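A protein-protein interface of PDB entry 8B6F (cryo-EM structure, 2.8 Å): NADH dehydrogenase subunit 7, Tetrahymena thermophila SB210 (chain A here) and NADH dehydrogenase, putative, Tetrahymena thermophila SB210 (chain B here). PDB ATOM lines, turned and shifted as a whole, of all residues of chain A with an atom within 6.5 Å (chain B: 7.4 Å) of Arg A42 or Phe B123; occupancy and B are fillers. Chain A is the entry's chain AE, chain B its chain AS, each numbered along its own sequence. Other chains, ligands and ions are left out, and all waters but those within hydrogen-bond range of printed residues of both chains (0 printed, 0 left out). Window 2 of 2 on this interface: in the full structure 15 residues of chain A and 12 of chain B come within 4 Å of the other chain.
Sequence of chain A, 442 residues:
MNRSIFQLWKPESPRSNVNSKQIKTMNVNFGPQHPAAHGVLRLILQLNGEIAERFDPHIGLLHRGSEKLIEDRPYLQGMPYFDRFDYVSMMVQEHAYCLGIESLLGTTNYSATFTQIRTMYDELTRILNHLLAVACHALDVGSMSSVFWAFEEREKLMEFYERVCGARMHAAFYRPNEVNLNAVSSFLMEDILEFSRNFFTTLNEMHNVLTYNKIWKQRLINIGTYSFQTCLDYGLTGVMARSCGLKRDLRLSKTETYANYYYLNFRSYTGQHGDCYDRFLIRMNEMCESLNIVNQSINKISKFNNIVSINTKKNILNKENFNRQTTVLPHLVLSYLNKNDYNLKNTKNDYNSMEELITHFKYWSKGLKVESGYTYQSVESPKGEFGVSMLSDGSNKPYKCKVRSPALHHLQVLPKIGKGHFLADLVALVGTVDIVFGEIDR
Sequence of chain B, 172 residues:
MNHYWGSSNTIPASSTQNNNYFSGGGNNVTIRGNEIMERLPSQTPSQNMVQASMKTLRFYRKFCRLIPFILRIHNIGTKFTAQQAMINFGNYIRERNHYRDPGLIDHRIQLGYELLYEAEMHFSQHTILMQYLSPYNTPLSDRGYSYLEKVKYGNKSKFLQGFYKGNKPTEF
Printed residues of chain B that touch a printed residue of chain A: Ile B36, Met B37, His B122 and Phe B123.
Printed residues of chain A that touch a printed residue of chain B: Arg A42, Ile A44, Asp A56 and His A58.
Along chain A the printed residues that touch a printed residue of chain B span positions 42 to 58.
Among the printed residues, no Asp or Glu carboxylate lies within 4 Å of a Lys or Arg side-chain nitrogen of the other chain.
The backbone carbonyl oxygen of Phe B123 lies within hydrogen-bond range of the guanidinium group of Arg A42 (3.3 Å).
O of Met B37 sits close to OD2 of Asp A56.
Among the printed residues, merely in contact across the chains: Ile A44 with Ile B36, His A58 with Phe B123, Arg A42 with His B122, Ile A44 with Phe B123 and Asp A56 with Ile B36.
N of Ile A44 sits at hydrogen-bond distance from O of Asp A56, 2.9 Å away.
N of Phe B123 is in hydrogen-bond range of O of Glu B118 (3.0 Å).
The side-chain amide oxygen (OD1) of Asn A29 lies within hydrogen-bond range of the guanidinium group (NE) of Arg A42 (3.2 Å).
The side-chain hydroxyl (OH) of Tyr B117 is in hydrogen-bond range of the backbone NH (N) of Met B37, 2.9 Å away.
O of Arg A42 lies within hydrogen-bond range of N of His A58, at 2.9 Å.
Printed residues of chain B within 4 Å of Asp A56: Ile B36 and Met B37.
Of the printed residues of chain A, His B122 touches Arg A42.
The nearest residue of chain B that does not touch Arg A42 is Met B121 (4.8 Å).
The nearest residue of chain A that does not touch Phe B123 is Asp A56 (4.8 Å).
The nearest printed residue of chain A that does not touch His B122 is Asn A29 (6.7 Å).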
ATOM      1  N   ASN A  29      23.193   2.879  -8.060  1.00  0.00           N
ATOM      2  CA  ASN A  29      21.816   2.646  -7.630  1.00  0.00           C
ATOM      3  C   ASN A  29      21.052   3.958  -7.777  1.00  0.00           C
ATOM      4  O   ASN A  29      20.845   4.703  -6.821  1.00  0.00           O
ATOM      5  CB  ASN A  29      21.768   2.131  -6.196  1.00  0.00           C
ATOM      6  CG  ASN A  29      22.236   0.697  -6.074  1.00  0.00           C
ATOM      7  OD1 ASN A  29      21.427  -0.229  -6.068  1.00  0.00           O
ATOM      8  ND2 ASN A  29      23.545   0.506  -5.976  1.00  0.00           N
ATOM      9  N   PHE A  30      20.637   4.242  -9.009  1.00  0.00           N
ATOM     10  CA  PHE A  30      19.811   5.413  -9.265  1.00  0.00           C
ATOM     11  C   PHE A  30      18.508   5.277  -8.489  1.00  0.00           C
ATOM     12  O   PHE A  30      17.677   4.421  -8.805  1.00  0.00           O
ATOM     13  CB  PHE A  30      19.554   5.551 -10.768  1.00  0.00           C
ATOM     14  CG  PHE A  30      18.753   6.760 -11.147  1.00  0.00           C
ATOM     15  CD1 PHE A  30      19.378   7.971 -11.391  1.00  0.00           C
ATOM     16  CD2 PHE A  30      17.377   6.679 -11.281  1.00  0.00           C
ATOM     17  CE1 PHE A  30      18.641   9.085 -11.748  1.00  0.00           C
ATOM     18  CE2 PHE A  30      16.635   7.789 -11.638  1.00  0.00           C
ATOM     19  CZ  PHE A  30      17.268   8.993 -11.874  1.00  0.00           C
ATOM     20  N   GLY A  31      18.318   6.120  -7.478  1.00  0.00           N
ATOM     21  CA  GLY A  31      17.199   5.984  -6.580  1.00  0.00           C
ATOM     22  C   GLY A  31      17.441   4.898  -5.551  1.00  0.00           C
ATOM     23  O   GLY A  31      18.520   4.302  -5.487  1.00  0.00           O
ATOM     24  N   PRO A  32      16.433   4.617  -4.717  1.00  0.00           N
ATOM     25  CA  PRO A  32      15.116   5.270  -4.667  1.00  0.00           C
ATOM     26  C   PRO A  32      15.188   6.700  -4.155  1.00  0.00           C
ATOM     27  O   PRO A  32      14.454   7.565  -4.617  1.00  0.00           O
ATOM     28  CB  PRO A  32      14.323   4.374  -3.706  1.00  0.00           C
ATOM     29  CG  PRO A  32      15.360   3.720  -2.846  1.00  0.00           C
ATOM     30  CD  PRO A  32      16.540   3.515  -3.746  1.00  0.00           C
ATOM     31  N   ALA A  37      14.701  10.408  -9.522  1.00  0.00           N
ATOM     32  CA  ALA A  37      13.777   9.300  -9.345  1.00  0.00           C
ATOM     33  C   ALA A  37      12.578   9.744  -8.516  1.00  0.00           C
ATOM     34  O   ALA A  37      12.711  10.532  -7.576  1.00  0.00           O
ATOM     35  CB  ALA A  37      14.476   8.122  -8.669  1.00  0.00           C
ATOM     36  N   VAL A  40      10.609   5.613  -5.529  1.00  0.00           N
ATOM     37  CA  VAL A  40      10.468   4.184  -5.277  1.00  0.00           C
ATOM     38  C   VAL A  40      11.040   3.386  -6.440  1.00  0.00           C
ATOM     39  O   VAL A  40      10.658   2.231  -6.658  1.00  0.00           O
ATOM     40  CB  VAL A  40       8.996   3.818  -5.025  1.00  0.00           C
ATOM     41  CG1 VAL A  40       8.524   4.442  -3.731  1.00  0.00           C
ATOM     42  CG2 VAL A  40       8.127   4.274  -6.187  1.00  0.00           C
ATOM     43  N   LEU A  41      11.954   3.989  -7.192  1.00  0.00           N
ATOM     44  CA  LEU A  41      12.617   3.323  -8.304  1.00  0.00           C
ATOM     45  C   LEU A  41      14.059   3.051  -7.912  1.00  0.00           C
ATOM     46  O   LEU A  41      14.801   3.983  -7.587  1.00  0.00           O
ATOM     47  CB  LEU A  41      12.562   4.180  -9.568  1.00  0.00           C
ATOM     48  CG  LEU A  41      13.265   3.607 -10.803  1.00  0.00           C
ATOM     49  CD1 LEU A  41      12.607   2.313 -11.251  1.00  0.00           C
ATOM     50  CD2 LEU A  41      13.288   4.617 -11.937  1.00  0.00           C
ATOM     51  N   ARG A  42      14.453   1.785  -7.941  1.00  0.00           N
ATOM     52  CA  ARG A  42      15.834   1.390  -7.694  1.00  0.00           C
ATOM     53  C   ARG A  42      16.381   0.874  -9.020  1.00  0.00           C
ATOM     54  O   ARG A  42      16.297  -0.315  -9.324  1.00  0.00           O
ATOM     55  CB  ARG A  42      15.924   0.339  -6.597  1.00  0.00           C
ATOM     56  CG  ARG A  42      17.347  -0.044  -6.240  1.00  0.00           C
ATOM     57  CD  ARG A  42      17.380  -1.080  -5.132  1.00  0.00           C
ATOM     58  NE  ARG A  42      18.744  -1.491  -4.826  1.00  0.00           N
ATOM     59  CZ  ARG A  42      19.069  -2.392  -3.912  1.00  0.00           C
ATOM     60  NH1 ARG A  42      18.148  -3.006  -3.188  1.00  0.00           N
ATOM     61  NH2 ARG A  42      20.351  -2.684  -3.717  1.00  0.00           N
ATOM     62  N   LEU A  43      16.929   1.786  -9.813  1.00  0.00           N
ATOM     63  CA  LEU A  43      17.452   1.457 -11.133  1.00  0.00           C
ATOM     64  C   LEU A  43      18.945   1.194 -11.000  1.00  0.00           C
ATOM     65  O   LEU A  43      19.714   2.105 -10.677  1.00  0.00           O
ATOM     66  CB  LEU A  43      17.166   2.591 -12.114  1.00  0.00           C
ATOM     67  CG  LEU A  43      17.700   2.437 -13.539  1.00  0.00           C
ATOM     68  CD1 LEU A  43      16.975   1.324 -14.268  1.00  0.00           C
ATOM     69  CD2 LEU A  43      17.570   3.745 -14.295  1.00  0.00           C
ATOM     70  N   ILE A  44      19.361  -0.045 -11.241  1.00  0.00           N
ATOM     71  CA  ILE A  44      20.782  -0.364 -11.318  1.00  0.00           C
ATOM     72  C   ILE A  44      21.263   0.067 -12.698  1.00  0.00           C
ATOM     73  O   ILE A  44      20.887  -0.527 -13.710  1.00  0.00           O
ATOM     74  CB  ILE A  44      21.052  -1.851 -11.068  1.00  0.00           C
ATOM     75  CG1 ILE A  44      20.209  -2.366  -9.897  1.00  0.00           C
ATOM     76  CG2 ILE A  44      22.528  -2.079 -10.792  1.00  0.00           C
ATOM     77  CD1 ILE A  44      20.351  -1.552  -8.624  1.00  0.00           C
ATOM     78  N   ASP A  56      18.766  -2.143 -15.063  1.00  0.00           N
ATOM     79  CA  ASP A  56      18.088  -3.178 -14.284  1.00  0.00           C
ATOM     80  C   ASP A  56      17.166  -2.466 -13.305  1.00  0.00           C
ATOM     81  O   ASP A  56      17.555  -2.185 -12.163  1.00  0.00           O
ATOM     82  CB  ASP A  56      19.085  -4.079 -13.563  1.00  0.00           C
ATOM     83  CG  ASP A  56      18.440  -5.323 -12.992  1.00  0.00           C
ATOM     84  OD1 ASP A  56      17.219  -5.301 -12.739  1.00  0.00           O
ATOM     85  OD2 ASP A  56      19.157  -6.325 -12.789  1.00  0.00           O
ATOM     86  N   PRO A  57      15.937  -2.159 -13.713  1.00  0.00           N
ATOM     87  CA  PRO A  57      15.012  -1.475 -12.803  1.00  0.00           C
ATOM     88  C   PRO A  57      14.374  -2.432 -11.810  1.00  0.00           C
ATOM     89  O   PRO A  57      13.959  -3.541 -12.157  1.00  0.00           O
ATOM     90  CB  PRO A  57      13.960  -0.871 -13.746  1.00  0.00           C
ATOM     91  CG  PRO A  57      14.506  -1.040 -15.134  1.00  0.00           C
ATOM     92  CD  PRO A  57      15.406  -2.221 -15.082  1.00  0.00           C
ATOM     93  N   HIS A  58      14.303  -1.988 -10.558  1.00  0.00           N
ATOM     94  CA  HIS A  58      13.501  -2.636  -9.529  1.00  0.00           C
ATOM     95  C   HIS A  58      12.405  -1.663  -9.128  1.00  0.00           C
ATOM     96  O   HIS A  58      12.692  -0.529  -8.731  1.00  0.00           O
ATOM     97  CB  HIS A  58      14.347  -3.028  -8.316  1.00  0.00           C
ATOM     98  CG  HIS A  58      15.598  -3.773  -8.663  1.00  0.00           C
ATOM     99  ND1 HIS A  58      15.586  -5.057  -9.162  1.00  0.00           N
ATOM    100  CD2 HIS A  58      16.900  -3.419  -8.571  1.00  0.00           C
ATOM    101  CE1 HIS A  58      16.827  -5.459  -9.369  1.00  0.00           C
ATOM    102  NE2 HIS A  58      17.644  -4.484  -9.018  1.00  0.00           N
ATOM    103  N   ILE A  59      11.153  -2.107  -9.231  1.00  0.00           N
ATOM    104  CA  ILE A  59       9.991  -1.252  -9.050  1.00  0.00           C
ATOM    105  C   ILE A  59       9.085  -1.741  -7.927  1.00  0.00           C
ATOM    106  O   ILE A  59       7.979  -1.231  -7.765  1.00  0.00           O
ATOM    107  CB  ILE A  59       9.201  -1.116 -10.366  1.00  0.00           C
ATOM    108  CG1 ILE A  59       8.850  -2.502 -10.911  1.00  0.00           C
ATOM    109  CG2 ILE A  59      10.013  -0.327 -11.380  1.00  0.00           C
ATOM    110  CD1 ILE A  59       7.973  -2.482 -12.140  1.00  0.00           C
ATOM    111  N   LEU A  61       9.431  -1.309  -4.762  1.00  0.00           N
ATOM    112  CA  LEU A  61       9.525  -0.514  -3.546  1.00  0.00           C
ATOM    113  C   LEU A  61       8.209   0.157  -3.178  1.00  0.00           C
ATOM    114  O   LEU A  61       8.107   0.717  -2.082  1.00  0.00           O
ATOM    115  CB  LEU A  61      10.622   0.540  -3.693  1.00  0.00           C
ATOM    116  CG  LEU A  61      12.017   0.011  -4.041  1.00  0.00           C
ATOM    117  CD1 LEU A  61      13.016   1.149  -4.091  1.00  0.00           C
ATOM    118  CD2 LEU A  61      12.475  -1.048  -3.055  1.00  0.00           C
ATOM    119  N   PHE A 437       4.741   5.831  -9.879  1.00  0.00           N
ATOM    120  CA  PHE A 437       4.889   4.422  -9.546  1.00  0.00           C
ATOM    121  C   PHE A 437       3.731   3.868  -8.731  1.00  0.00           C
ATOM    122  O   PHE A 437       3.705   2.660  -8.471  1.00  0.00           O
ATOM    123  CB  PHE A 437       6.210   4.208  -8.810  1.00  0.00           C
ATOM    124  CG  PHE A 437       7.408   4.428  -9.679  1.00  0.00           C
ATOM    125  CD1 PHE A 437       7.888   5.706  -9.905  1.00  0.00           C
ATOM    126  CD2 PHE A 437       8.026   3.362 -10.308  1.00  0.00           C
ATOM    127  CE1 PHE A 437       8.980   5.915 -10.720  1.00  0.00           C
ATOM    128  CE2 PHE A 437       9.118   3.564 -11.127  1.00  0.00           C
ATOM    129  CZ  PHE A 437       9.594   4.844 -11.334  1.00  0.00           C
ATOM    130  N   ILE B  36      26.198  -5.773 -15.096  1.00  0.00           N
ATOM    131  CA  ILE B  36      25.030  -6.204 -14.334  1.00  0.00           C
ATOM    132  C   ILE B  36      24.209  -7.170 -15.176  1.00  0.00           C
ATOM    133  O   ILE B  36      24.402  -7.272 -16.392  1.00  0.00           O
ATOM    134  CB  ILE B  36      24.175  -5.006 -13.881  1.00  0.00           C
ATOM    135  CG1 ILE B  36      23.642  -4.235 -15.094  1.00  0.00           C
ATOM    136  CG2 ILE B  36      24.994  -4.101 -12.971  1.00  0.00           C
ATOM    137  CD1 ILE B  36      22.706  -3.096 -14.741  1.00  0.00           C
ATOM    138  N   MET B  37      23.286  -7.883 -14.533  1.00  0.00           N
ATOM    139  CA  MET B  37      22.438  -8.862 -15.206  1.00  0.00           C
ATOM    140  C   MET B  37      21.202  -8.149 -15.742  1.00  0.00           C
ATOM    141  O   MET B  37      20.320  -7.756 -14.973  1.00  0.00           O
ATOM    142  CB  MET B  37      22.055  -9.983 -14.243  1.00  0.00           C
ATOM    143  CG  MET B  37      21.173 -11.058 -14.856  1.00  0.00           C
ATOM    144  SD  MET B  37      20.690 -12.314 -13.657  1.00  0.00           S
ATOM    145  CE  MET B  37      22.256 -13.127 -13.359  1.00  0.00           C
ATOM    146  N   HIS B  74      28.865  -9.404   3.168  1.00  0.00           N
ATOM    147  CA  HIS B  74      27.771  -9.135   4.092  1.00  0.00           C
ATOM    148  C   HIS B  74      28.200  -9.145   5.552  1.00  0.00           C
ATOM    149  O   HIS B  74      27.370  -8.871   6.424  1.00  0.00           O
ATOM    150  CB  HIS B  74      26.644 -10.153   3.891  1.00  0.00           C
ATOM    151  CG  HIS B  74      25.893  -9.971   2.610  1.00  0.00           C
ATOM    152  ND1 HIS B  74      24.975  -8.959   2.424  1.00  0.00           N
ATOM    153  CD2 HIS B  74      25.920 -10.670   1.453  1.00  0.00           C
ATOM    154  CE1 HIS B  74      24.473  -9.042   1.205  1.00  0.00           C
ATOM    155  NE2 HIS B  74      25.029 -10.073   0.595  1.00  0.00           N
ATOM    156  N   GLU B 114      18.031 -16.405  -8.935  1.00  0.00           N
ATOM    157  CA  GLU B 114      17.692 -15.002  -8.729  1.00  0.00           C
ATOM    158  C   GLU B 114      18.104 -14.537  -7.338  1.00  0.00           C
ATOM    159  O   GLU B 114      18.711 -13.472  -7.182  1.00  0.00           O
ATOM    160  CB  GLU B 114      16.193 -14.801  -8.938  1.00  0.00           C
ATOM    161  CG  GLU B 114      15.709 -13.399  -8.633  1.00  0.00           C
ATOM    162  CD  GLU B 114      14.208 -13.294  -8.694  1.00  0.00           C
ATOM    163  OE1 GLU B 114      13.560 -14.279  -9.102  1.00  0.00           O
ATOM    164  OE2 GLU B 114      13.674 -12.228  -8.332  1.00  0.00           O
ATOM    165  N   LEU B 115      17.777 -15.321  -6.309  1.00  0.00           N
ATOM    166  CA  LEU B 115      18.114 -14.915  -4.948  1.00  0.00           C
ATOM    167  C   LEU B 115      19.621 -14.915  -4.737  1.00  0.00           C
ATOM    168  O   LEU B 115      20.153 -14.069  -4.011  1.00  0.00           O
ATOM    169  CB  LEU B 115      17.419 -15.817  -3.930  1.00  0.00           C
ATOM    170  CG  LEU B 115      15.884 -15.814  -3.946  1.00  0.00           C
ATOM    171  CD1 LEU B 115      15.338 -16.472  -2.694  1.00  0.00           C
ATOM    172  CD2 LEU B 115      15.308 -14.417  -4.112  1.00  0.00           C
ATOM    173  N   TYR B 117      21.833 -14.200  -7.055  1.00  0.00           N
ATOM    174  CA  TYR B 117      22.296 -12.970  -7.687  1.00  0.00           C
ATOM    175  C   TYR B 117      22.022 -11.763  -6.801  1.00  0.00           C
ATOM    176  O   TYR B 117      22.859 -10.858  -6.692  1.00  0.00           O
ATOM    177  CB  TYR B 117      21.629 -12.797  -9.048  1.00  0.00           C
ATOM    178  CG  TYR B 117      21.982 -11.502  -9.737  1.00  0.00           C
ATOM    179  CD1 TYR B 117      23.158 -11.377 -10.461  1.00  0.00           C
ATOM    180  CD2 TYR B 117      21.135 -10.405  -9.668  1.00  0.00           C
ATOM    181  CE1 TYR B 117      23.483 -10.197 -11.094  1.00  0.00           C
ATOM    182  CE2 TYR B 117      21.452  -9.220 -10.299  1.00  0.00           C
ATOM    183  CZ  TYR B 117      22.626  -9.124 -11.011  1.00  0.00           C
ATOM    184  OH  TYR B 117      22.947  -7.944 -11.640  1.00  0.00           O
ATOM    185  N   GLU B 118      20.852 -11.725  -6.163  1.00  0.00           N
ATOM    186  CA  GLU B 118      20.551 -10.636  -5.240  1.00  0.00           C
ATOM    187  C   GLU B 118      21.566 -10.586  -4.107  1.00  0.00           C
ATOM    188  O   GLU B 118      22.049  -9.508  -3.744  1.00  0.00           O
ATOM    189  CB  GLU B 118      19.137 -10.795  -4.685  1.00  0.00           C
ATOM    190  CG  GLU B 118      18.043 -10.630  -5.724  1.00  0.00           C
ATOM    191  CD  GLU B 118      16.668 -10.929  -5.164  1.00  0.00           C
ATOM    192  OE1 GLU B 118      16.570 -11.220  -3.955  1.00  0.00           O
ATOM    193  OE2 GLU B 118      15.685 -10.873  -5.934  1.00  0.00           O
ATOM    194  N   ALA B 119      21.896 -11.742  -3.531  1.00  0.00           N
ATOM    195  CA  ALA B 119      22.887 -11.775  -2.461  1.00  0.00           C
ATOM    196  C   ALA B 119      24.241 -11.271  -2.946  1.00  0.00           C
ATOM    197  O   ALA B 119      24.921 -10.520  -2.237  1.00  0.00           O
ATOM    198  CB  ALA B 119      23.012 -13.194  -1.908  1.00  0.00           C
ATOM    199  N   GLU B 120      24.648 -11.667  -4.154  1.00  0.00           N
ATOM    200  CA  GLU B 120      25.911 -11.184  -4.706  1.00  0.00           C
ATOM    201  C   GLU B 120      25.912  -9.669  -4.847  1.00  0.00           C
ATOM    202  O   GLU B 120      26.893  -9.004  -4.497  1.00  0.00           O
ATOM    203  CB  GLU B 120      26.166 -11.815  -6.075  1.00  0.00           C
ATOM    204  CG  GLU B 120      26.313 -13.320  -6.086  1.00  0.00           C
ATOM    205  CD  GLU B 120      26.286 -13.874  -7.497  1.00  0.00           C
ATOM    206  OE1 GLU B 120      26.956 -13.290  -8.374  1.00  0.00           O
ATOM    207  OE2 GLU B 120      25.585 -14.878  -7.735  1.00  0.00           O
ATOM    208  N   MET B 121      24.824  -9.105  -5.361  1.00  0.00           N
ATOM    209  CA  MET B 121      24.754  -7.695  -5.710  1.00  0.00           C
ATOM    210  C   MET B 121      24.261  -6.818  -4.569  1.00  0.00           C
ATOM    211  O   MET B 121      24.020  -5.627  -4.783  1.00  0.00           O
ATOM    212  CB  MET B 121      23.846  -7.507  -6.927  1.00  0.00           C
ATOM    213  CG  MET B 121      24.480  -7.915  -8.242  1.00  0.00           C
ATOM    214  SD  MET B 121      25.862  -6.857  -8.711  1.00  0.00           S
ATOM    215  CE  MET B 121      26.290  -7.550 -10.305  1.00  0.00           C
ATOM    216  N   HIS B 122      24.094  -7.373  -3.370  1.00  0.00           N
ATOM    217  CA  HIS B 122      23.691  -6.616  -2.189  1.00  0.00           C
ATOM    218  C   HIS B 122      22.264  -6.098  -2.294  1.00  0.00           C
ATOM    219  O   HIS B 122      21.885  -5.170  -1.572  1.00  0.00           O
ATOM    220  CB  HIS B 122      24.644  -5.446  -1.914  1.00  0.00           C
ATOM    221  CG  HIS B 122      25.790  -5.798  -1.018  1.00  0.00           C
ATOM    222  ND1 HIS B 122      25.642  -5.993   0.338  1.00  0.00           N
ATOM    223  CD2 HIS B 122      27.106  -5.976  -1.282  1.00  0.00           C
ATOM    224  CE1 HIS B 122      26.814  -6.283   0.869  1.00  0.00           C
ATOM    225  NE2 HIS B 122      27.720  -6.279  -0.092  1.00  0.00           N
ATOM    226  N   PHE B 123      21.454  -6.672  -3.186  1.00  0.00           N
ATOM    227  CA  PHE B 123      20.055  -6.274  -3.262  1.00  0.00           C
ATOM    228  C   PHE B 123      19.330  -6.580  -1.959  1.00  0.00           C
ATOM    229  O   PHE B 123      18.458  -5.816  -1.529  1.00  0.00           O
ATOM    230  CB  PHE B 123      19.369  -6.977  -4.436  1.00  0.00           C
ATOM    231  CG  PHE B 123      19.911  -6.590  -5.786  1.00  0.00           C
ATOM    232  CD1 PHE B 123      20.737  -5.487  -5.940  1.00  0.00           C
ATOM    233  CD2 PHE B 123      19.581  -7.329  -6.908  1.00  0.00           C
ATOM    234  CE1 PHE B 123      21.225  -5.136  -7.183  1.00  0.00           C
ATOM    235  CE2 PHE B 123      20.067  -6.983  -8.153  1.00  0.00           C
ATOM    236  CZ  PHE B 123      20.889  -5.885  -8.291  1.00  0.00           C
ATOM    237  N   SER B 124      19.679  -7.687  -1.314  1.00  0.00           N
ATOM    238  CA  SER B 124      19.082  -8.088  -0.051  1.00  0.00           C
ATOM    239  C   SER B 124      19.956  -7.649   1.118  1.00  0.00           C
ATOM    240  O   SER B 124      21.135  -7.324   0.957  1.00  0.00           O
ATOM    241  CB  SER B 124      18.879  -9.605  -0.008  1.00  0.00           C
ATOM    242  OG  SER B 124      18.240 -10.068  -1.184  1.00  0.00           O
ATOM    243  N   GLN B 125      19.357  -7.636   2.304  1.00  0.00           N
ATOM    244  CA  GLN B 125      20.076  -7.326   3.531  1.00  0.00           C
ATOM    245  C   GLN B 125      20.607  -8.610   4.155  1.00  0.00           C
ATOM    246  O   GLN B 125      20.041  -9.690   3.973  1.00  0.00           O
ATOM    247  CB  GLN B 125      19.166  -6.598   4.522  1.00  0.00           C
ATOM    248  CG  GLN B 125      19.903  -5.962   5.688  1.00  0.00           C
ATOM    249  CD  GLN B 125      20.818  -4.839   5.253  1.00  0.00           C
ATOM    250  OE1 GLN B 125      20.642  -4.260   4.184  1.00  0.00           O
ATOM    251  NE2 GLN B 125      21.806  -4.528   6.082  1.00  0.00           N
ATOM    252  N   LEU B 129      18.606 -12.192   4.486  1.00  0.00           N
ATOM    253  CA  LEU B 129      19.012 -13.327   3.669  1.00  0.00           C
ATOM    254  C   LEU B 129      19.696 -14.432   4.461  1.00  0.00           C
ATOM    255  O   LEU B 129      19.830 -15.545   3.946  1.00  0.00           O
ATOM    256  CB  LEU B 129      19.947 -12.857   2.544  1.00  0.00           C
ATOM    257  CG  LEU B 129      21.330 -12.320   2.929  1.00  0.00           C
ATOM    258  CD1 LEU B 129      22.370 -13.429   3.047  1.00  0.00           C
ATOM    259  CD2 LEU B 129      21.788 -11.274   1.930  1.00  0.00           C
